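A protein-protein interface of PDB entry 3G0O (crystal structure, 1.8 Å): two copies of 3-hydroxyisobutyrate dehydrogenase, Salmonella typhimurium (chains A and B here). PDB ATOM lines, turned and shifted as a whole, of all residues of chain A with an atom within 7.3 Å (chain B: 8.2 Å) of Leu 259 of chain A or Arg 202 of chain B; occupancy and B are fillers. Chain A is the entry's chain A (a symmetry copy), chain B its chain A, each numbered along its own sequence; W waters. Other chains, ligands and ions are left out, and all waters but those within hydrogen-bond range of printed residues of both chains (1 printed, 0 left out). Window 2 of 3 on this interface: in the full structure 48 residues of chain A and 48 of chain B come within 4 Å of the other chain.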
ATOM      1  N   THR A 177      24.046   6.952   1.297  1.00  0.00           N
ATOM      2  CA  THR A 177      23.316   5.893   0.603  1.00  0.00           C
ATOM      3  C   THR A 177      24.103   5.473  -0.636  1.00  0.00           C
ATOM      4  O   THR A 177      24.190   4.285  -0.962  1.00  0.00           O
ATOM      5  CB  THR A 177      21.908   6.361   0.176  1.00  0.00           C
ATOM      6  OG1 THR A 177      21.106   6.571   1.344  1.00  0.00           O
ATOM      7  CG2 THR A 177      21.235   5.309  -0.712  1.00  0.00           C
ATOM      8  N   ILE A 181      25.913   1.693  -1.530  1.00  0.00           N
ATOM      9  CA  ILE A 181      25.776   0.947  -2.771  1.00  0.00           C
ATOM     10  C   ILE A 181      27.167   0.702  -3.358  1.00  0.00           C
ATOM     11  O   ILE A 181      27.467  -0.392  -3.835  1.00  0.00           O
ATOM     12  CB  ILE A 181      24.891   1.711  -3.771  1.00  0.00           C
ATOM     13  CG1 ILE A 181      23.500   1.906  -3.162  1.00  0.00           C
ATOM     14  CG2 ILE A 181      24.800   0.944  -5.083  1.00  0.00           C
ATOM     15  CD1 ILE A 181      22.564   2.732  -4.000  1.00  0.00           C
ATOM     16  N   ALA A 253      23.485  -4.917   3.691  1.00  0.00           N
ATOM     17  CA  ALA A 253      22.420  -5.860   4.017  1.00  0.00           C
ATOM     18  C   ALA A 253      21.228  -5.149   4.672  1.00  0.00           C
ATOM     19  O   ALA A 253      20.079  -5.357   4.275  1.00  0.00           O
ATOM     20  CB  ALA A 253      22.956  -6.954   4.942  1.00  0.00           C
ATOM     21  N   ASP A 254      21.505  -4.308   5.666  1.00  0.00           N
ATOM     22  CA  ASP A 254      20.454  -3.568   6.362  1.00  0.00           C
ATOM     23  C   ASP A 254      19.690  -2.649   5.415  1.00  0.00           C
ATOM     24  O   ASP A 254      18.462  -2.579   5.467  1.00  0.00           O
ATOM     25  CB  ASP A 254      21.040  -2.727   7.497  1.00  0.00           C
ATOM     26  CG  ASP A 254      21.538  -3.567   8.652  1.00  0.00           C
ATOM     27  OD1 ASP A 254      21.096  -4.726   8.794  1.00  0.00           O
ATOM     28  OD2 ASP A 254      22.365  -3.056   9.435  1.00  0.00           O
ATOM     29  N   THR A 255      20.419  -1.941   4.556  1.00  0.00           N
ATOM     30  CA  THR A 255      19.794  -1.029   3.602  1.00  0.00           C
ATOM     31  C   THR A 255      18.830  -1.787   2.689  1.00  0.00           C
ATOM     32  O   THR A 255      17.690  -1.370   2.487  1.00  0.00           O
ATOM     33  CB  THR A 255      20.860  -0.306   2.741  1.00  0.00           C
ATOM     34  OG1 THR A 255      21.677   0.514   3.585  1.00  0.00           O
ATOM     35  CG2 THR A 255      20.201   0.571   1.684  1.00  0.00           C
ATOM     36  N   ALA A 256      19.290  -2.909   2.146  1.00  0.00           N
ATOM     37  CA  ALA A 256      18.458  -3.711   1.261  1.00  0.00           C
ATOM     38  C   ALA A 256      17.246  -4.290   1.988  1.00  0.00           C
ATOM     39  O   ALA A 256      16.134  -4.281   1.458  1.00  0.00           O
ATOM     40  CB  ALA A 256      19.285  -4.841   0.643  1.00  0.00           C
ATOM     41  N   LYS A 257      17.451  -4.792   3.202  1.00  0.00           N
ATOM     42  CA  LYS A 257      16.335  -5.373   3.939  1.00  0.00           C
ATOM     43  C   LYS A 257      15.259  -4.329   4.232  1.00  0.00           C
ATOM     44  O   LYS A 257      14.063  -4.611   4.131  1.00  0.00           O
ATOM     45  CB  LYS A 257      16.820  -6.025   5.238  1.00  0.00           C
ATOM     46  CG  LYS A 257      15.721  -6.787   5.971  1.00  0.00           C
ATOM     47  CD  LYS A 257      16.272  -7.934   6.813  1.00  0.00           C
ATOM     48  CE  LYS A 257      17.117  -7.437   7.967  1.00  0.00           C
ATOM     49  NZ  LYS A 257      16.320  -6.592   8.895  1.00  0.00           N
ATOM     50  N   ALA A 258      15.680  -3.117   4.576  1.00  0.00           N
ATOM     51  CA  ALA A 258      14.729  -2.047   4.859  1.00  0.00           C
ATOM     52  C   ALA A 258      13.896  -1.753   3.612  1.00  0.00           C
ATOM     53  O   ALA A 258      12.747  -1.329   3.712  1.00  0.00           O
ATOM     54  CB  ALA A 258      15.471  -0.790   5.308  1.00  0.00           C
ATOM     55  N   LEU A 259      14.486  -1.982   2.439  1.00  0.00           N
ATOM     56  CA  LEU A 259      13.809  -1.753   1.163  1.00  0.00           C
ATOM     57  C   LEU A 259      13.153  -3.021   0.618  1.00  0.00           C
ATOM     58  O   LEU A 259      12.606  -3.009  -0.485  1.00  0.00           O
ATOM     59  CB  LEU A 259      14.806  -1.240   0.120  1.00  0.00           C
ATOM     60  CG  LEU A 259      15.449   0.118   0.391  1.00  0.00           C
ATOM     61  CD1 LEU A 259      16.633   0.346  -0.553  1.00  0.00           C
ATOM     62  CD2 LEU A 259      14.397   1.202   0.212  1.00  0.00           C
ATOM     63  N   ARG A 260      13.208  -4.107   1.383  1.00  0.00           N
ATOM     64  CA  ARG A 260      12.632  -5.375   0.937  1.00  0.00           C
ATOM     65  C   ARG A 260      13.222  -5.711  -0.436  1.00  0.00           C
ATOM     66  O   ARG A 260      12.504  -6.033  -1.376  1.00  0.00           O
ATOM     67  CB  ARG A 260      11.104  -5.264   0.841  1.00  0.00           C
ATOM     68  CG  ARG A 260      10.404  -6.571   0.490  1.00  0.00           C
ATOM     69  CD  ARG A 260       8.896  -6.380   0.420  1.00  0.00           C
ATOM     70  NE  ARG A 260       8.283  -6.333   1.741  1.00  0.00           N
ATOM     71  CZ  ARG A 260       7.841  -7.400   2.395  1.00  0.00           C
ATOM     72  NH1 ARG A 260       7.936  -8.607   1.849  1.00  0.00           N
ATOM     73  NH2 ARG A 260       7.308  -7.264   3.600  1.00  0.00           N
ATOM     74  N   PHE A 261      14.545  -5.632  -0.534  1.00  0.00           N
ATOM     75  CA  PHE A 261      15.256  -5.902  -1.785  1.00  0.00           C
ATOM     76  C   PHE A 261      16.249  -7.044  -1.553  1.00  0.00           C
ATOM     77  O   PHE A 261      17.019  -7.011  -0.593  1.00  0.00           O
ATOM     78  CB  PHE A 261      16.010  -4.642  -2.214  1.00  0.00           C
ATOM     79  CG  PHE A 261      16.630  -4.735  -3.577  1.00  0.00           C
ATOM     80  CD1 PHE A 261      15.887  -4.434  -4.714  1.00  0.00           C
ATOM     81  CD2 PHE A 261      17.951  -5.133  -3.726  1.00  0.00           C
ATOM     82  CE1 PHE A 261      16.459  -4.520  -5.979  1.00  0.00           C
ATOM     83  CE2 PHE A 261      18.531  -5.224  -4.987  1.00  0.00           C
ATOM     84  CZ  PHE A 261      17.784  -4.921  -6.114  1.00  0.00           C
ATOM     85  N   PRO A 262      16.262  -8.055  -2.442  1.00  0.00           N
ATOM     86  CA  PRO A 262      17.177  -9.194  -2.291  1.00  0.00           C
ATOM     87  C   PRO A 262      18.573  -8.943  -2.845  1.00  0.00           C
ATOM     88  O   PRO A 262      18.726  -8.270  -3.868  1.00  0.00           O
ATOM     89  CB  PRO A 262      16.464 -10.297  -3.055  1.00  0.00           C
ATOM     90  CG  PRO A 262      15.929  -9.528  -4.255  1.00  0.00           C
ATOM     91  CD  PRO A 262      15.383  -8.242  -3.612  1.00  0.00           C
ATOM     92  N   GLU B 195      23.055  -6.095  -9.787  1.00  0.00           N
ATOM     93  CA  GLU B 195      22.517  -6.116  -8.436  1.00  0.00           C
ATOM     94  C   GLU B 195      22.635  -4.737  -7.797  1.00  0.00           C
ATOM     95  O   GLU B 195      21.676  -4.235  -7.207  1.00  0.00           O
ATOM     96  CB  GLU B 195      23.258  -7.159  -7.591  1.00  0.00           C
ATOM     97  CG  GLU B 195      22.746  -7.297  -6.164  1.00  0.00           C
ATOM     98  CD  GLU B 195      23.323  -8.515  -5.474  1.00  0.00           C
ATOM     99  OE1 GLU B 195      23.163  -9.632  -6.012  1.00  0.00           O
ATOM    100  OE2 GLU B 195      23.936  -8.356  -4.399  1.00  0.00           O
ATOM    101  N   ALA B 196      23.802  -4.118  -7.935  1.00  0.00           N
ATOM    102  CA  ALA B 196      24.041  -2.797  -7.358  1.00  0.00           C
ATOM    103  C   ALA B 196      23.175  -1.698  -7.976  1.00  0.00           C
ATOM    104  O   ALA B 196      22.671  -0.828  -7.266  1.00  0.00           O
ATOM    105  CB  ALA B 196      25.511  -2.434  -7.490  1.00  0.00           C
ATOM    106  N   MET B 197      22.994  -1.740  -9.291  1.00  0.00           N
ATOM    107  CA  MET B 197      22.183  -0.721  -9.957  1.00  0.00           C
ATOM    108  C   MET B 197      20.701  -0.896  -9.646  1.00  0.00           C
ATOM    109  O   MET B 197      19.980   0.080  -9.509  1.00  0.00           O
ATOM    110  CB  MET B 197      22.422  -0.743 -11.471  1.00  0.00           C
ATOM    111  CG  MET B 197      23.805  -0.251 -11.871  1.00  0.00           C
ATOM    112  SD  MET B 197      24.095   1.649 -11.455  1.00  0.00           S
ATOM    113  CE  MET B 197      23.818   2.358 -13.227  1.00  0.00           C
ATOM    114  N   ALA B 198      20.245  -2.143  -9.533  1.00  0.00           N
ATOM    115  CA  ALA B 198      18.846  -2.383  -9.207  1.00  0.00           C
ATOM    116  C   ALA B 198      18.598  -1.860  -7.789  1.00  0.00           C
ATOM    117  O   ALA B 198      17.556  -1.272  -7.508  1.00  0.00           O
ATOM    118  CB  ALA B 198      18.524  -3.879  -9.291  1.00  0.00           C
ATOM    119  N   LEU B 199      19.552  -2.083  -6.890  1.00  0.00           N
ATOM    120  CA  LEU B 199      19.411  -1.591  -5.523  1.00  0.00           C
ATOM    121  C   LEU B 199      19.395  -0.062  -5.538  1.00  0.00           C
ATOM    122  O   LEU B 199      18.634   0.565  -4.808  1.00  0.00           O
ATOM    123  CB  LEU B 199      20.568  -2.070  -4.640  1.00  0.00           C
ATOM    124  CG  LEU B 199      20.606  -1.443  -3.238  1.00  0.00           C
ATOM    125  CD1 LEU B 199      19.336  -1.796  -2.473  1.00  0.00           C
ATOM    126  CD2 LEU B 199      21.844  -1.930  -2.487  1.00  0.00           C
ATOM    127  N   ALA B 200      20.249   0.527  -6.371  1.00  0.00           N
ATOM    128  CA  ALA B 200      20.328   1.981  -6.489  1.00  0.00           C
ATOM    129  C   ALA B 200      18.978   2.529  -6.926  1.00  0.00           C
ATOM    130  O   ALA B 200      18.507   3.536  -6.397  1.00  0.00           O
ATOM    131  CB  ALA B 200      21.400   2.368  -7.500  1.00  0.00           C
ATOM    132  N   ALA B 201      18.359   1.858  -7.890  1.00  0.00           N
ATOM    133  CA  ALA B 201      17.057   2.280  -8.394  1.00  0.00           C
ATOM    134  C   ALA B 201      16.031   2.191  -7.270  1.00  0.00           C
ATOM    135  O   ALA B 201      15.249   3.118  -7.052  1.00  0.00           O
ATOM    136  CB  ALA B 201      16.635   1.400  -9.565  1.00  0.00           C
ATOM    137  N   ARG B 202      16.048   1.070  -6.558  1.00  0.00           N
ATOM    138  CA  ARG B 202      15.119   0.844  -5.456  1.00  0.00           C
ATOM    139  C   ARG B 202      15.283   1.882  -4.350  1.00  0.00           C
ATOM    140  O   ARG B 202      14.308   2.285  -3.710  1.00  0.00           O
ATOM    141  CB  ARG B 202      15.328  -0.555  -4.871  1.00  0.00           C
ATOM    142  CG  ARG B 202      14.433  -0.869  -3.676  1.00  0.00           C
ATOM    143  CD  ARG B 202      12.968  -0.906  -4.082  1.00  0.00           C
ATOM    144  NE  ARG B 202      12.077  -1.116  -2.940  1.00  0.00           N
ATOM    145  CZ  ARG B 202      11.664  -0.158  -2.111  1.00  0.00           C
ATOM    146  NH1 ARG B 202      12.055   1.101  -2.286  1.00  0.00           N
ATOM    147  NH2 ARG B 202      10.856  -0.460  -1.102  1.00  0.00           N
ATOM    148  N   ALA B 203      16.522   2.313  -4.138  1.00  0.00           N
ATOM    149  CA  ALA B 203      16.842   3.293  -3.112  1.00  0.00           C
ATOM    150  C   ALA B 203      16.538   4.717  -3.568  1.00  0.00           C
ATOM    151  O   ALA B 203      16.627   5.659  -2.781  1.00  0.00           O
ATOM    152  CB  ALA B 203      18.310   3.175  -2.726  1.00  0.00           C
ATOM    153  N   GLY B 204      16.189   4.871  -4.840  1.00  0.00           N
ATOM    154  CA  GLY B 204      15.865   6.185  -5.360  1.00  0.00           C
ATOM    155  C   GLY B 204      17.037   7.015  -5.844  1.00  0.00           C
ATOM    156  O   GLY B 204      16.935   8.238  -5.918  1.00  0.00           O
ATOM    157  N   ILE B 205      18.153   6.365  -6.167  1.00  0.00           N
ATOM    158  CA  ILE B 205      19.328   7.070  -6.662  1.00  0.00           C
ATOM    159  C   ILE B 205      19.301   7.045  -8.190  1.00  0.00           C
ATOM    160  O   ILE B 205      19.153   5.980  -8.789  1.00  0.00           O
ATOM    161  CB  ILE B 205      20.646   6.390  -6.203  1.00  0.00           C
ATOM    162  CG1 ILE B 205      20.697   6.298  -4.675  1.00  0.00           C
ATOM    163  CG2 ILE B 205      21.846   7.160  -6.752  1.00  0.00           C
ATOM    164  CD1 ILE B 205      20.639   7.643  -3.963  1.00  0.00           C
ATOM    165  N   LEU B 207      20.194   6.462 -11.793  1.00  0.00           N
ATOM    166  CA  LEU B 207      21.174   5.518 -12.324  1.00  0.00           C
ATOM    167  C   LEU B 207      22.349   6.165 -13.048  1.00  0.00           C
ATOM    168  O   LEU B 207      23.473   5.660 -12.981  1.00  0.00           O
ATOM    169  CB  LEU B 207      20.489   4.503 -13.244  1.00  0.00           C
ATOM    170  CG  LEU B 207      19.415   3.627 -12.587  1.00  0.00           C
ATOM    171  CD1 LEU B 207      19.000   2.528 -13.556  1.00  0.00           C
ATOM    172  CD2 LEU B 207      19.950   3.024 -11.302  1.00  0.00           C
ATOM    173  N   PHE B 293      15.358  -8.598 -10.943  1.00  0.00           N
ATOM    174  CA  PHE B 293      15.069  -7.799  -9.759  1.00  0.00           C
ATOM    175  C   PHE B 293      13.751  -7.045  -9.912  1.00  0.00           C
ATOM    176  O   PHE B 293      13.100  -6.777  -8.881  1.00  0.00           O
ATOM    177  CB  PHE B 293      16.220  -6.818  -9.501  1.00  0.00           C
ATOM    178  CG  PHE B 293      17.488  -7.485  -9.041  1.00  0.00           C
ATOM    179  CD1 PHE B 293      17.612  -7.938  -7.729  1.00  0.00           C
ATOM    180  CD2 PHE B 293      18.542  -7.696  -9.925  1.00  0.00           C
ATOM    181  CE1 PHE B 293      18.777  -8.592  -7.300  1.00  0.00           C
ATOM    182  CE2 PHE B 293      19.706  -8.347  -9.509  1.00  0.00           C
ATOM    183  CZ  PHE B 293      19.819  -8.797  -8.193  1.00  0.00           C
HETATM  184  O   HOH W   1      12.235  -3.999  -3.133  1.00  0.00           O
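Printed residues of chain B within 4 Å of Ile 181 of chain A: Ala 196 (3.5 Å) and Ala 200 (3.4 Å).
Leu 259 of chain A touches three residues of chain B.
Of the printed residues of chain A, Ala 198 of chain B touches Phe 261 (3.4 Å).
Arg 202 of chain B touches just these residues of chain A: Leu 259 and Phe 261.
Gly 204 of chain B touches none of the printed residues of chain A.
The nearest residue of chain B that does not touch Leu 259 of chain A is Gly 204 of chain B (6.2 Å).
The nearest residue of chain A that does not touch Arg 202 of chain B is Arg 260 of chain A (5.0 Å).
The nearest printed residue of chain A that does not touch Ala 196 of chain B is Phe 261 of chain A (6.1 Å).
O of Ala 256 of chain A sits at hydrogen-bond distance from N of Phe 261 of chain A, at 2.9 Å.
The backbone carbonyl oxygen (O) of Ala 200 of chain B lies within hydrogen-bond range of the backbone NH (N) of Ile 205 of chain B.
No position is printed for both chains.
Of the 11 pairs that touch across the chains among the printed residues, none has its exchanged pair printed and touching as well.
Ala 196 of chain B touches Ile 181 of chain A.
Ala 200 of chain B touches Ile 181 of chain A.
Leu 259 of chain A touches Leu 199 of chain B.
CA of Ala 203 of chain B touches CD1 of Leu 259 of chain A, 3.9 Å away.
CE2 of Phe 261 of chain A touches O of Glu 195 of chain B (3.97 Å).
CZ of Phe 261 of chain A touches CB of Ala 198 of chain B, at 3.4 Å.
Leu 199 of chain B touches Phe 261 of chain A.
Phe 261 of chain A touches Arg 202 of chain B.
Phe 261 of chain A touches Phe 293 of chain B (CZ to CD1, 3.4 Å).
CE1 of Phe 293 of chain B touches O of Pro 262 of chain A (3.4 Å).
Of the 12 printed residues of chain A, 4 touch a printed residue of chain B.
Printed residues of chain A that touch a printed residue of chain B: Ile 181, Leu 259, Phe 261 and Pro 262.
Printed residues of chain B that touch a printed residue of chain A: Glu 195, Ala 196, Ala 198, Leu 199, Ala 200, Arg 202, Ala 203 and Phe 293.
Hydrophobic or aromatic side chains of chain B within 4 Å of the printed part of chain A: Ala 198, Leu 199, Ala 200, Ala 203 and Phe 293.
Along chain B the printed residues that touch a printed residue of chain A span positions 195 to 293.
Water W1 lies within hydrogen-bond range of the backbone carbonyl oxygen of Arg 260 of chain A (2.7 Å), the backbone carbonyl oxygen of Leu 259 of chain A (2.9 Å) and the guanidinium group of Arg 202 of chain B (2.9 Å).
NE of Arg 202 of chain B sits at hydrogen-bond distance from O of Leu 259 of chain A (3.1 Å).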
